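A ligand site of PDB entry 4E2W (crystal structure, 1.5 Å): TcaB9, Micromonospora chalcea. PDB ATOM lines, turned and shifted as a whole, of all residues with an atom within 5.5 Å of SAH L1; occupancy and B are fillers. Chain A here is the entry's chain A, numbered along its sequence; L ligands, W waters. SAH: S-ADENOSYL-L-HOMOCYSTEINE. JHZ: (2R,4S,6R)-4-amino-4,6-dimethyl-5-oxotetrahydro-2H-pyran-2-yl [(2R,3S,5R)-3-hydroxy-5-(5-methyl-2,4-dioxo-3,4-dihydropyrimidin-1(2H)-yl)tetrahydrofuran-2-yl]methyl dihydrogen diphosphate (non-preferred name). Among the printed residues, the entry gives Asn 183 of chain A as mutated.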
ATOM      1  N   ARG A  70      -8.807  -7.638  17.089  1.00  0.00           N
ATOM      2  CA  ARG A  70      -9.728  -7.283  16.008  1.00  0.00           C
ATOM      3  C   ARG A  70      -9.265  -6.198  15.048  1.00  0.00           C
ATOM      4  O   ARG A  70      -9.484  -6.327  13.847  1.00  0.00           O
ATOM      5  CB  ARG A  70     -11.135  -7.020  16.541  1.00  0.00           C
ATOM      6  CG  ARG A  70     -11.221  -5.795  17.442  1.00  0.00           C
ATOM      7  CD  ARG A  70     -12.642  -5.697  17.955  1.00  0.00           C
ATOM      8  NE  ARG A  70     -12.844  -4.494  18.761  1.00  0.00           N
ATOM      9  CZ  ARG A  70     -13.999  -4.232  19.354  1.00  0.00           C
ATOM     10  NH1 ARG A  70     -15.055  -5.015  19.217  1.00  0.00           N
ATOM     11  NH2 ARG A  70     -14.094  -3.123  20.098  1.00  0.00           N
ATOM     12  N   PHE A  74      -9.574  -6.222  10.880  1.00  0.00           N
ATOM     13  CA  PHE A  74     -10.742  -5.509  10.380  1.00  0.00           C
ATOM     14  C   PHE A  74     -10.536  -4.009  10.610  1.00  0.00           C
ATOM     15  O   PHE A  74     -10.333  -3.605  11.741  1.00  0.00           O
ATOM     16  CB  PHE A  74     -11.946  -6.055  11.137  1.00  0.00           C
ATOM     17  CG  PHE A  74     -12.095  -7.555  11.080  1.00  0.00           C
ATOM     18  CD1 PHE A  74     -12.229  -8.236   9.866  1.00  0.00           C
ATOM     19  CD2 PHE A  74     -12.108  -8.253  12.271  1.00  0.00           C
ATOM     20  CE1 PHE A  74     -12.344  -9.609   9.862  1.00  0.00           C
ATOM     21  CE2 PHE A  74     -12.238  -9.639  12.275  1.00  0.00           C
ATOM     22  CZ  PHE A  74     -12.377 -10.315  11.074  1.00  0.00           C
ATOM     23  N   TYR A  78      -9.524  -3.525   4.926  1.00  0.00           N
ATOM     24  CA  TYR A  78      -9.862  -4.939   4.744  1.00  0.00           C
ATOM     25  C   TYR A  78     -10.369  -5.264   3.328  1.00  0.00           C
ATOM     26  O   TYR A  78     -11.257  -4.548   2.814  1.00  0.00           O
ATOM     27  CB  TYR A  78     -10.948  -5.242   5.799  1.00  0.00           C
ATOM     28  CG  TYR A  78     -11.360  -6.701   5.833  1.00  0.00           C
ATOM     29  CD1 TYR A  78     -12.609  -7.082   5.369  1.00  0.00           C
ATOM     30  CD2 TYR A  78     -10.519  -7.671   6.349  1.00  0.00           C
ATOM     31  CE1 TYR A  78     -13.043  -8.420   5.429  1.00  0.00           C
ATOM     32  CE2 TYR A  78     -10.925  -9.006   6.393  1.00  0.00           C
ATOM     33  CZ  TYR A  78     -12.189  -9.362   5.953  1.00  0.00           C
ATOM     34  OH  TYR A  78     -12.651 -10.659   5.956  1.00  0.00           O
ATOM     35  N   TYR A  80     -11.712  -8.109   1.671  1.00  0.00           N
ATOM     36  CA  TYR A  80     -12.625  -9.140   1.142  1.00  0.00           C
ATOM     37  C   TYR A  80     -13.940  -8.522   0.678  1.00  0.00           C
ATOM     38  O   TYR A  80     -14.600  -7.808   1.440  1.00  0.00           O
ATOM     39  CB  TYR A  80     -13.007 -10.110   2.255  1.00  0.00           C
ATOM     40  CG  TYR A  80     -13.888 -11.220   1.727  1.00  0.00           C
ATOM     41  CD1 TYR A  80     -13.419 -12.114   0.766  1.00  0.00           C
ATOM     42  CD2 TYR A  80     -15.208 -11.356   2.193  1.00  0.00           C
ATOM     43  CE1 TYR A  80     -14.196 -13.137   0.213  1.00  0.00           C
ATOM     44  CE2 TYR A  80     -16.010 -12.374   1.661  1.00  0.00           C
ATOM     45  CZ  TYR A  80     -15.492 -13.233   0.703  1.00  0.00           C
ATOM     46  OH  TYR A  80     -16.236 -14.275   0.206  1.00  0.00           O
ATOM     47  N   SER A  82     -17.573  -9.452  -0.461  1.00  0.00           N
ATOM     48  CA  SER A  82     -18.487 -10.605  -0.557  1.00  0.00           C
ATOM     49  C   SER A  82     -19.081 -10.760  -1.964  1.00  0.00           C
ATOM     50  O   SER A  82     -19.304 -11.901  -2.437  1.00  0.00           O
ATOM     51  CB  SER A  82     -19.637 -10.456   0.449  1.00  0.00           C
ATOM     52  OG  SER A  82     -19.083 -10.271   1.725  1.00  0.00           O
ATOM     53  N   PHE A  92     -27.402 -15.100  -0.702  1.00  0.00           N
ATOM     54  CA  PHE A  92     -27.831 -14.130   0.314  1.00  0.00           C
ATOM     55  C   PHE A  92     -29.167 -13.460  -0.033  1.00  0.00           C
ATOM     56  O   PHE A  92     -29.935 -13.123   0.855  1.00  0.00           O
ATOM     57  CB  PHE A  92     -26.727 -13.116   0.603  1.00  0.00           C
ATOM     58  CG  PHE A  92     -25.601 -13.694   1.405  1.00  0.00           C
ATOM     59  CD1 PHE A  92     -25.844 -14.178   2.686  1.00  0.00           C
ATOM     60  CD2 PHE A  92     -24.325 -13.780   0.869  1.00  0.00           C
ATOM     61  CE1 PHE A  92     -24.839 -14.720   3.455  1.00  0.00           C
ATOM     62  CE2 PHE A  92     -23.294 -14.343   1.642  1.00  0.00           C
ATOM     63  CZ  PHE A  92     -23.550 -14.793   2.952  1.00  0.00           C
ATOM     64  N   GLU A 113     -27.797  -6.645  10.587  1.00  0.00           N
ATOM     65  CA  GLU A 113     -26.811  -7.634  10.187  1.00  0.00           C
ATOM     66  C   GLU A 113     -25.454  -7.272  10.795  1.00  0.00           C
ATOM     67  O   GLU A 113     -25.017  -6.115  10.814  1.00  0.00           O
ATOM     68  CB  GLU A 113     -26.702  -7.711   8.660  1.00  0.00           C
ATOM     69  CG  GLU A 113     -25.653  -8.728   8.224  1.00  0.00           C
ATOM     70  CD  GLU A 113     -25.563  -8.942   6.713  1.00  0.00           C
ATOM     71  OE1 GLU A 113     -25.022 -10.021   6.334  1.00  0.00           O
ATOM     72  OE2 GLU A 113     -25.996  -8.077   5.904  1.00  0.00           O
ATOM     73  N   ILE A 114     -24.833  -8.305  11.360  1.00  0.00           N
ATOM     74  CA  ILE A 114     -23.457  -8.217  11.880  1.00  0.00           C
ATOM     75  C   ILE A 114     -22.517  -8.661  10.771  1.00  0.00           C
ATOM     76  O   ILE A 114     -22.600  -9.794  10.308  1.00  0.00           O
ATOM     77  CB  ILE A 114     -23.299  -9.052  13.172  1.00  0.00           C
ATOM     78  CG1 ILE A 114     -24.411  -8.698  14.164  1.00  0.00           C
ATOM     79  CG2 ILE A 114     -21.831  -9.072  13.640  1.00  0.00           C
ATOM     80  CD1 ILE A 114     -24.461  -9.615  15.394  1.00  0.00           C
ATOM     81  N   GLY A 115     -21.673  -7.747  10.311  1.00  0.00           N
ATOM     82  CA  GLY A 115     -20.737  -8.041   9.212  1.00  0.00           C
ATOM     83  C   GLY A 115     -21.311  -7.899   7.823  1.00  0.00           C
ATOM     84  O   GLY A 115     -21.124  -8.811   6.998  1.00  0.00           O
ATOM     85  N   CYS A 116     -22.025  -6.803   7.541  1.00  0.00           N
ATOM     86  CA  CYS A 116     -22.687  -6.703   6.252  1.00  0.00           C
ATOM     87  C   CYS A 116     -21.759  -6.598   5.053  1.00  0.00           C
ATOM     88  O   CYS A 116     -22.226  -6.839   3.913  1.00  0.00           O
ATOM     89  CB  CYS A 116     -23.781  -5.627   6.243  1.00  0.00           C
ATOM     90  SG  CYS A 116     -23.060  -3.980   6.427  1.00  0.00           S
ATOM     91  N   ASN A 117     -20.469  -6.315   5.271  1.00  0.00           N
ATOM     92  CA  ASN A 117     -19.531  -6.213   4.152  1.00  0.00           C
ATOM     93  C   ASN A 117     -20.095  -5.210   3.150  1.00  0.00           C
ATOM     94  O   ASN A 117     -20.613  -4.138   3.549  1.00  0.00           O
ATOM     95  CB  ASN A 117     -19.153  -7.614   3.619  1.00  0.00           C
ATOM     96  CG  ASN A 117     -17.882  -7.587   2.786  1.00  0.00           C
ATOM     97  OD1 ASN A 117     -17.958  -7.441   1.570  1.00  0.00           O
ATOM     98  ND2 ASN A 117     -16.718  -7.749   3.423  1.00  0.00           N
ATOM     99  N   ILE A 120     -24.036  -7.360   0.416  1.00  0.00           N
ATOM    100  CA  ILE A 120     -24.523  -8.558  -0.311  1.00  0.00           C
ATOM    101  C   ILE A 120     -25.925  -9.045   0.113  1.00  0.00           C
ATOM    102  O   ILE A 120     -26.737  -9.551  -0.682  1.00  0.00           O
ATOM    103  CB  ILE A 120     -23.461  -9.700  -0.241  1.00  0.00           C
ATOM    104  CG1 ILE A 120     -23.819 -10.856  -1.204  1.00  0.00           C
ATOM    105  CG2 ILE A 120     -23.173 -10.235   1.193  1.00  0.00           C
ATOM    106  CD1 ILE A 120     -22.521 -11.593  -1.605  1.00  0.00           C
ATOM    107  N   PHE A 135     -23.801  -3.553  10.631  1.00  0.00           N
ATOM    108  CA  PHE A 135     -22.577  -3.289  11.390  1.00  0.00           C
ATOM    109  C   PHE A 135     -21.463  -3.794  10.488  1.00  0.00           C
ATOM    110  O   PHE A 135     -21.428  -4.964  10.099  1.00  0.00           O
ATOM    111  CB  PHE A 135     -22.514  -4.062  12.715  1.00  0.00           C
ATOM    112  CG  PHE A 135     -23.308  -3.410  13.801  1.00  0.00           C
ATOM    113  CD1 PHE A 135     -22.682  -2.574  14.715  1.00  0.00           C
ATOM    114  CD2 PHE A 135     -24.689  -3.614  13.916  1.00  0.00           C
ATOM    115  CE1 PHE A 135     -23.404  -1.962  15.741  1.00  0.00           C
ATOM    116  CE2 PHE A 135     -25.420  -2.998  14.920  1.00  0.00           C
ATOM    117  CZ  PHE A 135     -24.771  -2.161  15.842  1.00  0.00           C
ATOM    118  N   GLU A 136     -20.592  -2.854  10.152  1.00  0.00           N
ATOM    119  CA  GLU A 136     -19.460  -3.193   9.303  1.00  0.00           C
ATOM    120  C   GLU A 136     -18.275  -2.322   9.734  1.00  0.00           C
ATOM    121  O   GLU A 136     -18.162  -1.154   9.276  1.00  0.00           O
ATOM    122  CB  GLU A 136     -19.801  -2.961   7.814  1.00  0.00           C
ATOM    123  CG  GLU A 136     -18.671  -3.399   6.895  1.00  0.00           C
ATOM    124  CD  GLU A 136     -17.984  -4.642   7.445  1.00  0.00           C
ATOM    125  OE1 GLU A 136     -18.500  -5.754   7.189  1.00  0.00           O
ATOM    126  OE2 GLU A 136     -16.939  -4.539   8.124  1.00  0.00           O
ATOM    127  N   PRO A 137     -17.381  -2.885  10.560  1.00  0.00           N
ATOM    128  CA  PRO A 137     -16.321  -2.054  11.143  1.00  0.00           C
ATOM    129  C   PRO A 137     -15.194  -1.818  10.161  1.00  0.00           C
ATOM    130  O   PRO A 137     -14.267  -1.085  10.545  1.00  0.00           O
ATOM    131  CB  PRO A 137     -15.822  -2.916  12.310  1.00  0.00           C
ATOM    132  CG  PRO A 137     -16.145  -4.362  11.883  1.00  0.00           C
ATOM    133  CD  PRO A 137     -17.532  -4.129  11.330  1.00  0.00           C
ATOM    134  N   SER A 138     -15.241  -2.428   8.974  1.00  0.00           N
ATOM    135  CA  SER A 138     -14.194  -2.261   7.959  1.00  0.00           C
ATOM    136  C   SER A 138     -14.756  -1.204   7.024  1.00  0.00           C
ATOM    137  O   SER A 138     -15.693  -1.470   6.256  1.00  0.00           O
ATOM    138  CB  SER A 138     -13.903  -3.558   7.175  1.00  0.00           C
ATOM    139  OG  SER A 138     -13.260  -4.447   8.080  1.00  0.00           O
ATOM    140  N   VAL A 141     -15.239  -1.509   2.736  1.00  0.00           N
ATOM    141  CA  VAL A 141     -16.430  -2.231   2.298  1.00  0.00           C
ATOM    142  C   VAL A 141     -17.729  -1.653   2.842  1.00  0.00           C
ATOM    143  O   VAL A 141     -18.756  -1.681   2.150  1.00  0.00           O
ATOM    144  CB  VAL A 141     -16.274  -3.772   2.542  1.00  0.00           C
ATOM    145  CG1 VAL A 141     -15.108  -4.356   1.748  1.00  0.00           C
ATOM    146  CG2 VAL A 141     -16.073  -3.991   4.042  1.00  0.00           C
ATOM    147  N   ASP A 155     -18.809   0.161  12.938  1.00  0.00           N
ATOM    148  CA  ASP A 155     -18.478  -0.152  14.327  1.00  0.00           C
ATOM    149  C   ASP A 155     -18.566  -1.674  14.380  1.00  0.00           C
ATOM    150  O   ASP A 155     -19.250  -2.335  13.593  1.00  0.00           O
ATOM    151  CB  ASP A 155     -19.647   0.347  15.202  1.00  0.00           C
ATOM    152  CG  ASP A 155     -19.386   1.686  15.847  1.00  0.00           C
ATOM    153  OD1 ASP A 155     -20.358   2.475  15.848  1.00  0.00           O
ATOM    154  OD2 ASP A 155     -18.247   1.902  16.328  1.00  0.00           O
ATOM    155  N   PHE A 156     -17.870  -2.239  15.361  1.00  0.00           N
ATOM    156  CA  PHE A 156     -18.065  -3.628  15.724  1.00  0.00           C
ATOM    157  C   PHE A 156     -19.361  -3.732  16.517  1.00  0.00           C
ATOM    158  O   PHE A 156     -19.680  -2.917  17.393  1.00  0.00           O
ATOM    159  CB  PHE A 156     -16.931  -4.037  16.674  1.00  0.00           C
ATOM    160  CG  PHE A 156     -15.559  -4.047  15.999  1.00  0.00           C
ATOM    161  CD1 PHE A 156     -15.201  -5.090  15.147  1.00  0.00           C
ATOM    162  CD2 PHE A 156     -14.645  -3.008  16.183  1.00  0.00           C
ATOM    163  CE1 PHE A 156     -13.950  -5.118  14.507  1.00  0.00           C
ATOM    164  CE2 PHE A 156     -13.385  -3.039  15.564  1.00  0.00           C
ATOM    165  CZ  PHE A 156     -13.026  -4.082  14.713  1.00  0.00           C
ATOM    166  N   PHE A 157     -20.126  -4.774  16.203  1.00  0.00           N
ATOM    167  CA  PHE A 157     -21.214  -5.184  17.084  1.00  0.00           C
ATOM    168  C   PHE A 157     -20.660  -5.812  18.337  1.00  0.00           C
ATOM    169  O   PHE A 157     -19.780  -6.668  18.264  1.00  0.00           O
ATOM    170  CB  PHE A 157     -22.094  -6.210  16.341  1.00  0.00           C
ATOM    171  CG  PHE A 157     -23.339  -6.598  17.089  1.00  0.00           C
ATOM    172  CD1 PHE A 157     -23.306  -7.558  18.107  1.00  0.00           C
ATOM    173  CD2 PHE A 157     -24.564  -6.005  16.748  1.00  0.00           C
ATOM    174  CE1 PHE A 157     -24.479  -7.910  18.809  1.00  0.00           C
ATOM    175  CE2 PHE A 157     -25.737  -6.350  17.438  1.00  0.00           C
ATOM    176  CZ  PHE A 157     -25.692  -7.290  18.476  1.00  0.00           C
ATOM    177  N   GLU A 158     -21.171  -5.368  19.478  1.00  0.00           N
ATOM    178  CA  GLU A 158     -20.747  -5.872  20.811  1.00  0.00           C
ATOM    179  C   GLU A 158     -21.791  -5.346  21.791  1.00  0.00           C
ATOM    180  O   GLU A 158     -22.677  -4.629  21.352  1.00  0.00           O
ATOM    181  CB  GLU A 158     -19.334  -5.397  21.197  1.00  0.00           C
ATOM    182  CG  GLU A 158     -19.227  -3.875  21.118  1.00  0.00           C
ATOM    183  CD  GLU A 158     -17.876  -3.303  21.525  1.00  0.00           C
ATOM    184  OE1 GLU A 158     -17.669  -2.768  22.637  1.00  0.00           O
ATOM    185  OE2 GLU A 158     -16.970  -3.358  20.692  1.00  0.00           O
ATOM    186  N   ALA A 178     -23.380 -13.777   8.884  1.00  0.00           N
ATOM    187  CA  ALA A 178     -22.854 -14.869   8.047  1.00  0.00           C
ATOM    188  C   ALA A 178     -21.322 -14.757   7.987  1.00  0.00           C
ATOM    189  O   ALA A 178     -20.833 -13.655   7.686  1.00  0.00           O
ATOM    190  CB  ALA A 178     -23.428 -14.788   6.620  1.00  0.00           C
ATOM    191  N   ASN A 179     -20.599 -15.857   8.232  1.00  0.00           N
ATOM    192  CA  ASN A 179     -19.120 -15.826   8.089  1.00  0.00           C
ATOM    193  C   ASN A 179     -18.514 -14.718   8.957  1.00  0.00           C
ATOM    194  O   ASN A 179     -17.433 -14.212   8.603  1.00  0.00           O
ATOM    195  CB  ASN A 179     -18.718 -15.744   6.622  1.00  0.00           C
ATOM    196  CG  ASN A 179     -19.427 -16.862   5.867  1.00  0.00           C
ATOM    197  OD1 ASN A 179     -19.241 -18.012   6.261  1.00  0.00           O
ATOM    198  ND2 ASN A 179     -20.294 -16.531   4.903  1.00  0.00           N
ATOM    199  N   THR A 180     -19.144 -14.373  10.072  1.00  0.00           N
ATOM    200  CA  THR A 180     -18.744 -13.246  10.948  1.00  0.00           C
ATOM    201  C   THR A 180     -18.706 -13.696  12.417  1.00  0.00           C
ATOM    202  O   THR A 180     -17.759 -13.381  13.140  1.00  0.00           O
ATOM    203  CB  THR A 180     -19.734 -12.069  10.774  1.00  0.00           C
ATOM    204  OG1 THR A 180     -19.631 -11.670   9.412  1.00  0.00           O
ATOM    205  CG2 THR A 180     -19.227 -10.870  11.551  1.00  0.00           C
ATOM    206  N   ASN A 183     -15.740 -15.349  13.720  1.00  0.00           N
ATOM    207  CA  ASN A 183     -14.494 -14.566  13.710  1.00  0.00           C
ATOM    208  C   ASN A 183     -14.338 -13.854  15.059  1.00  0.00           C
ATOM    209  O   ASN A 183     -13.319 -13.191  15.289  1.00  0.00           O
ATOM    210  CB  ASN A 183     -14.563 -13.378  12.744  1.00  0.00           C
ATOM    211  CG  ASN A 183     -14.932 -13.649  11.325  1.00  0.00           C
ATOM    212  OD1 ASN A 183     -14.837 -12.723  10.509  1.00  0.00           O
ATOM    213  ND2 ASN A 183     -15.384 -14.865  10.962  1.00  0.00           N
ATOM    214  N   ILE A 184     -15.321 -13.920  15.943  1.00  0.00           N
ATOM    215  CA  ILE A 184     -15.385 -12.990  17.100  1.00  0.00           C
ATOM    216  C   ILE A 184     -15.151 -13.735  18.430  1.00  0.00           C
ATOM    217  O   ILE A 184     -16.015 -14.445  18.993  1.00  0.00           O
ATOM    218  CB  ILE A 184     -16.769 -12.293  17.154  1.00  0.00           C
ATOM    219  CG1 ILE A 184     -16.876 -11.362  15.920  1.00  0.00           C
ATOM    220  CG2 ILE A 184     -16.918 -11.442  18.431  1.00  0.00           C
ATOM    221  CD1 ILE A 184     -18.294 -10.822  15.659  1.00  0.00           C
ATOM    222  N   TYR A 186     -14.978 -12.525  21.332  1.00  0.00           N
ATOM    223  CA  TYR A 186     -15.777 -11.927  22.392  1.00  0.00           C
ATOM    224  C   TYR A 186     -17.256 -12.200  22.151  1.00  0.00           C
ATOM    225  O   TYR A 186     -18.117 -11.314  22.284  1.00  0.00           O
ATOM    226  CB  TYR A 186     -15.473 -10.419  22.533  1.00  0.00           C
ATOM    227  CG  TYR A 186     -15.441  -9.677  21.204  1.00  0.00           C
ATOM    228  CD1 TYR A 186     -14.328  -9.705  20.383  1.00  0.00           C
ATOM    229  CD2 TYR A 186     -16.570  -8.971  20.798  1.00  0.00           C
ATOM    230  CE1 TYR A 186     -14.325  -8.981  19.192  1.00  0.00           C
ATOM    231  CE2 TYR A 186     -16.597  -8.289  19.589  1.00  0.00           C
ATOM    232  CZ  TYR A 186     -15.470  -8.334  18.791  1.00  0.00           C
ATOM    233  OH  TYR A 186     -15.504  -7.663  17.601  1.00  0.00           O
ATOM    234  N   VAL A 190     -21.093 -10.327  22.275  1.00  0.00           N
ATOM    235  CA  VAL A 190     -22.063 -10.279  21.187  1.00  0.00           C
ATOM    236  C   VAL A 190     -23.403 -10.803  21.687  1.00  0.00           C
ATOM    237  O   VAL A 190     -24.425 -10.191  21.394  1.00  0.00           O
ATOM    238  CB  VAL A 190     -21.617 -11.098  19.940  1.00  0.00           C
ATOM    239  CG1 VAL A 190     -22.761 -11.194  18.917  1.00  0.00           C
ATOM    240  CG2 VAL A 190     -20.368 -10.474  19.331  1.00  0.00           C
ATOM    241  N   HIS A 256     -19.100 -22.118   1.061  1.00  0.00           N
ATOM    242  CA  HIS A 256     -17.876 -22.021   1.858  1.00  0.00           C
ATOM    243  C   HIS A 256     -17.327 -23.340   2.371  1.00  0.00           C
ATOM    244  O   HIS A 256     -16.769 -23.359   3.471  1.00  0.00           O
ATOM    245  CB  HIS A 256     -17.992 -20.951   2.945  1.00  0.00           C
ATOM    246  CG  HIS A 256     -18.084 -19.567   2.369  1.00  0.00           C
ATOM    247  ND1 HIS A 256     -17.077 -19.022   1.591  1.00  0.00           N
ATOM    248  CD2 HIS A 256     -19.061 -18.636   2.433  1.00  0.00           C
ATOM    249  CE1 HIS A 256     -17.450 -17.824   1.190  1.00  0.00           C
ATOM    250  NE2 HIS A 256     -18.637 -17.558   1.694  1.00  0.00           N
HETATM  251  N   SAH L   1     -21.423 -11.485   5.696  1.00  0.00           N
HETATM  252  CA  SAH L   1     -20.377 -11.386   4.639  1.00  0.00           C
HETATM  253  CB  SAH L   1     -19.006 -10.898   5.076  1.00  0.00           C
HETATM  254  CG  SAH L   1     -18.054 -11.832   5.802  1.00  0.00           C
HETATM  255  SD  SAH L   1     -16.504 -11.000   6.024  1.00  0.00           S
HETATM  256  C   SAH L   1     -20.269 -12.710   3.927  1.00  0.00           C
HETATM  257  O   SAH L   1     -20.760 -13.707   4.485  1.00  0.00           O
HETATM  258  OXT SAH L   1     -19.677 -12.781   2.850  1.00  0.00           O
HETATM  259  C5' SAH L   1     -16.592 -10.786   7.785  1.00  0.00           C
HETATM  260  C4' SAH L   1     -17.008  -9.340   8.065  1.00  0.00           C
HETATM  261  O4' SAH L   1     -17.168  -9.275   9.493  1.00  0.00           O
HETATM  262  C3' SAH L   1     -15.877  -8.382   7.717  1.00  0.00           C
HETATM  263  O3' SAH L   1     -16.349  -7.449   6.735  1.00  0.00           O
HETATM  264  C2' SAH L   1     -15.562  -7.691   9.040  1.00  0.00           C
HETATM  265  O2' SAH L   1     -15.241  -6.298   8.934  1.00  0.00           O
HETATM  266  C1' SAH L   1     -16.862  -7.904   9.816  1.00  0.00           C
HETATM  267  N9  SAH L   1     -16.735  -7.894  11.303  1.00  0.00           N
HETATM  268  C8  SAH L   1     -15.745  -8.351  12.076  1.00  0.00           C
HETATM  269  N7  SAH L   1     -16.017  -8.231  13.400  1.00  0.00           N
HETATM  270  C5  SAH L   1     -17.277  -7.713  13.464  1.00  0.00           C
HETATM  271  C6  SAH L   1     -18.191  -7.319  14.549  1.00  0.00           C
HETATM  272  N6  SAH L   1     -17.875  -7.433  15.855  1.00  0.00           N
HETATM  273  N1  SAH L   1     -19.343  -6.781  14.114  1.00  0.00           N
HETATM  274  C2  SAH L   1     -19.719  -6.615  12.843  1.00  0.00           C
HETATM  275  N3  SAH L   1     -18.972  -6.960  11.800  1.00  0.00           N
HETATM  276  C4  SAH L   1     -17.751  -7.494  12.087  1.00  0.00           C
HETATM  277  P   JHZ L   2     -13.511 -16.778  -0.534  1.00  0.00           P
HETATM  278  C1  JHZ L   2     -12.945 -14.558   3.280  1.00  0.00           C
HETATM  279  O1  JHZ L   2     -12.405 -15.880   3.200  1.00  0.00           O
HETATM  280  C2  JHZ L   2     -12.458 -13.914   4.595  1.00  0.00           C
HETATM  281  P2  JHZ L   2     -11.807 -16.328   1.780  1.00  0.00           P
HETATM  282  C3  JHZ L   2     -13.554 -14.403   5.568  1.00  0.00           C
HETATM  283  N3  JHZ L   2     -12.972 -14.671   6.887  1.00  0.00           N
HETATM  284  C4  JHZ L   2     -14.434 -15.596   5.213  1.00  0.00           C
HETATM  285  O4  JHZ L   2     -14.755 -16.497   5.976  1.00  0.00           O
HETATM  286  C5  JHZ L   2     -15.018 -15.724   3.856  1.00  0.00           C
HETATM  287  O5  JHZ L   2     -14.375 -14.660   3.152  1.00  0.00           O
HETATM  288  C6  JHZ L   2     -16.528 -15.516   3.682  1.00  0.00           C
HETATM  289  C1X JHZ L   2     -11.453 -14.853  -5.704  1.00  0.00           C
HETATM  290  N11 JHZ L   2     -12.361 -15.305  -6.763  1.00  0.00           N
HETATM  291  O1P JHZ L   2     -14.933 -16.262  -0.793  1.00  0.00           O
HETATM  292  C2X JHZ L   2     -12.093 -13.708  -4.931  1.00  0.00           C
HETATM  293  C21 JHZ L   2     -11.993 -15.206  -8.053  1.00  0.00           C
HETATM  294  O21 JHZ L   2     -10.837 -14.823  -8.352  1.00  0.00           O
HETATM  295  O2P JHZ L   2     -13.330 -18.271  -0.728  1.00  0.00           O
HETATM  296  C3X JHZ L   2     -11.655 -13.887  -3.487  1.00  0.00           C
HETATM  297  O3X JHZ L   2     -10.413 -13.183  -3.254  1.00  0.00           O
HETATM  298  N31 JHZ L   2     -12.829 -15.682  -9.021  1.00  0.00           N
HETATM  299  C3M JHZ L   2     -14.546 -13.234   5.622  1.00  0.00           C
HETATM  300  O3P JHZ L   2     -11.179 -17.692   1.830  1.00  0.00           O
HETATM  301  C4X JHZ L   2     -11.329 -15.384  -3.438  1.00  0.00           C
HETATM  302  O4X JHZ L   2     -11.247 -15.898  -4.752  1.00  0.00           O
HETATM  303  C41 JHZ L   2     -14.096 -16.078  -8.794  1.00  0.00           C
HETATM  304  O41 JHZ L   2     -14.806 -16.445  -9.755  1.00  0.00           O
HETATM  305  O4P JHZ L   2     -10.916 -15.221   1.281  1.00  0.00           O
HETATM  306  C5X JHZ L   2     -12.398 -16.296  -2.879  1.00  0.00           C
HETATM  307  O5X JHZ L   2     -12.437 -16.039  -1.475  1.00  0.00           O
HETATM  308  C51 JHZ L   2     -14.571 -16.212  -7.390  1.00  0.00           C
HETATM  309  C5A JHZ L   2     -15.951 -16.713  -7.009  1.00  0.00           C
HETATM  310  C61 JHZ L   2     -13.605 -15.776  -6.483  1.00  0.00           C
HETATM  311  OPP JHZ L   2     -13.193 -16.238   0.954  1.00  0.00           O
HETATM  312  O   HOH W   1     -19.479 -14.866   1.261  1.00  0.00           O
HETATM  313  O   HOH W   2     -23.852 -11.414   4.385  1.00  0.00           O
HETATM  314  O   HOH W   3     -14.100  -8.426  15.514  1.00  0.00           O
HETATM  315  O   HOH W   4     -23.153 -11.145   8.011  1.00  0.00           O
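O2' of SAH L1 is in hydrogen-bond range of OE2 of Glu 136, 2.6 Å away.
The side-chain hydroxyl of Ser 82 is in hydrogen-bond range of an oxygen (OXT) of SAH L1, 2.8 Å away.
The side-chain hydroxyl of Ser 138 sits at hydrogen-bond distance from an oxygen (O2') of SAH L1.
ND2 of Asn 179 is in hydrogen-bond range of O of SAH L1, at 2.9 Å.
The side-chain hydroxyl (OH) of Tyr 186 is in hydrogen-bond range of a nitrogen (N6) of SAH L1 (3.0 Å).
The backbone NH (N) of Gly 115 is in hydrogen-bond range of a nitrogen (N3) of SAH L1 (3.2 Å).
A nitrogen (N) of SAH L1 sits at hydrogen-bond distance from the backbone carbonyl oxygen (O) of Gly 115 (3.0 Å).
A nitrogen (N1) of SAH L1 sits at hydrogen-bond distance from the backbone NH of Phe 157.
A nitrogen (N6) of SAH L1 sits at hydrogen-bond distance from the backbone carbonyl oxygen (O) of Phe 157.
N of SAH L1 sits at hydrogen-bond distance from O of Ala 178 (3.0 Å).
O4' of SAH L1 sits close to OG1 of Thr 180, 3.4 Å away.
The side-chain amide nitrogen (ND2) of Asn 117 is in hydrogen-bond range of an oxygen (O3') of SAH L1 (3.3 Å).
OE1 of Glu 113 lies within salt-bridge range of N of SAH L1 (3.9 Å).
An oxygen (O1P) of JHZ L2 lies within hydrogen-bond range of the side-chain hydroxyl (OH) of Tyr 80, 2.6 Å away.
Water W1 lies within hydrogen-bond range of an oxygen (OXT) of SAH L1 (2.6 Å), a ring nitrogen (NE2) of His 256 (2.9 Å) and the side-chain hydroxyl (OH) of Tyr 80 (3.5 Å).
Water W2 bridges OE1 of Glu 113 (2.7 Å) and N of SAH L1 (2.8 Å).
Water W3 lies within hydrogen-bond range of OH of Tyr 186 (2.6 Å) and N7 of SAH L1 (2.9 Å).
OE2 of Glu 136 is in hydrogen-bond range of N of Ser 138 (2.8 Å).
OE1 of Glu 136 sits at hydrogen-bond distance from N of Asn 117 (2.8 Å).
OD1 of Asn 117 is in hydrogen-bond range of N of Ser 82, at 2.9 Å.
The backbone carbonyl oxygen (O) of Asn 179 sits at hydrogen-bond distance from the side-chain amide nitrogen (ND2) of Asn 183.
N of Gly 115 lies within hydrogen-bond range of O of Phe 135, 2.8 Å away.
O of Ala 178 is in hydrogen-bond range of OG1 of Thr 180, at 2.9 Å.
O of Glu 113 lies within hydrogen-bond range of N of Phe 135 (2.8 Å).
The backbone carbonyl oxygen of Phe 135 lies within hydrogen-bond range of the backbone NH of Cys 116 (3.2 Å).
Phe 74 touches SAH L1.
CE1 of Tyr 78 touches C3' of SAH L1, at 3.6 Å.
CE2 of Tyr 80 touches OXT of SAH L1 (3.9 Å).
Phe 92 touches SAH L1 (CZ to O, 3.4 Å).
Ile 114 touches SAH L1.
Phe 135 touches SAH L1.
CD of Pro 137 touches N3 of SAH L1, 3.2 Å away.
Phe 156 touches SAH L1.
Asn 183 touches SAH L1 (OD1 to C5', 3.8 Å).
CD1 of Ile 184 touches N6 of SAH L1, at 3.4 Å.
Hydrophobic or aromatic side chains that line SAH L1: Phe 74, Tyr 78, Tyr 80, Phe 92, Ile 114, Phe 135, Pro 137, Phe 156, Phe 157, Ala 178, Ile 184 and Tyr 186.
21 residues have an atom within 4 Å of SAH L1: Phe 74, Tyr 78, Tyr 80, Ser 82, Phe 92, Glu 113, Ile 114, Gly 115, Asn 117, Phe 135, Glu 136, Pro 137, Ser 138, Phe 156, Phe 157, Ala 178, Asn 179, Thr 180, Asn 183, Ile 184 and Tyr 186.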
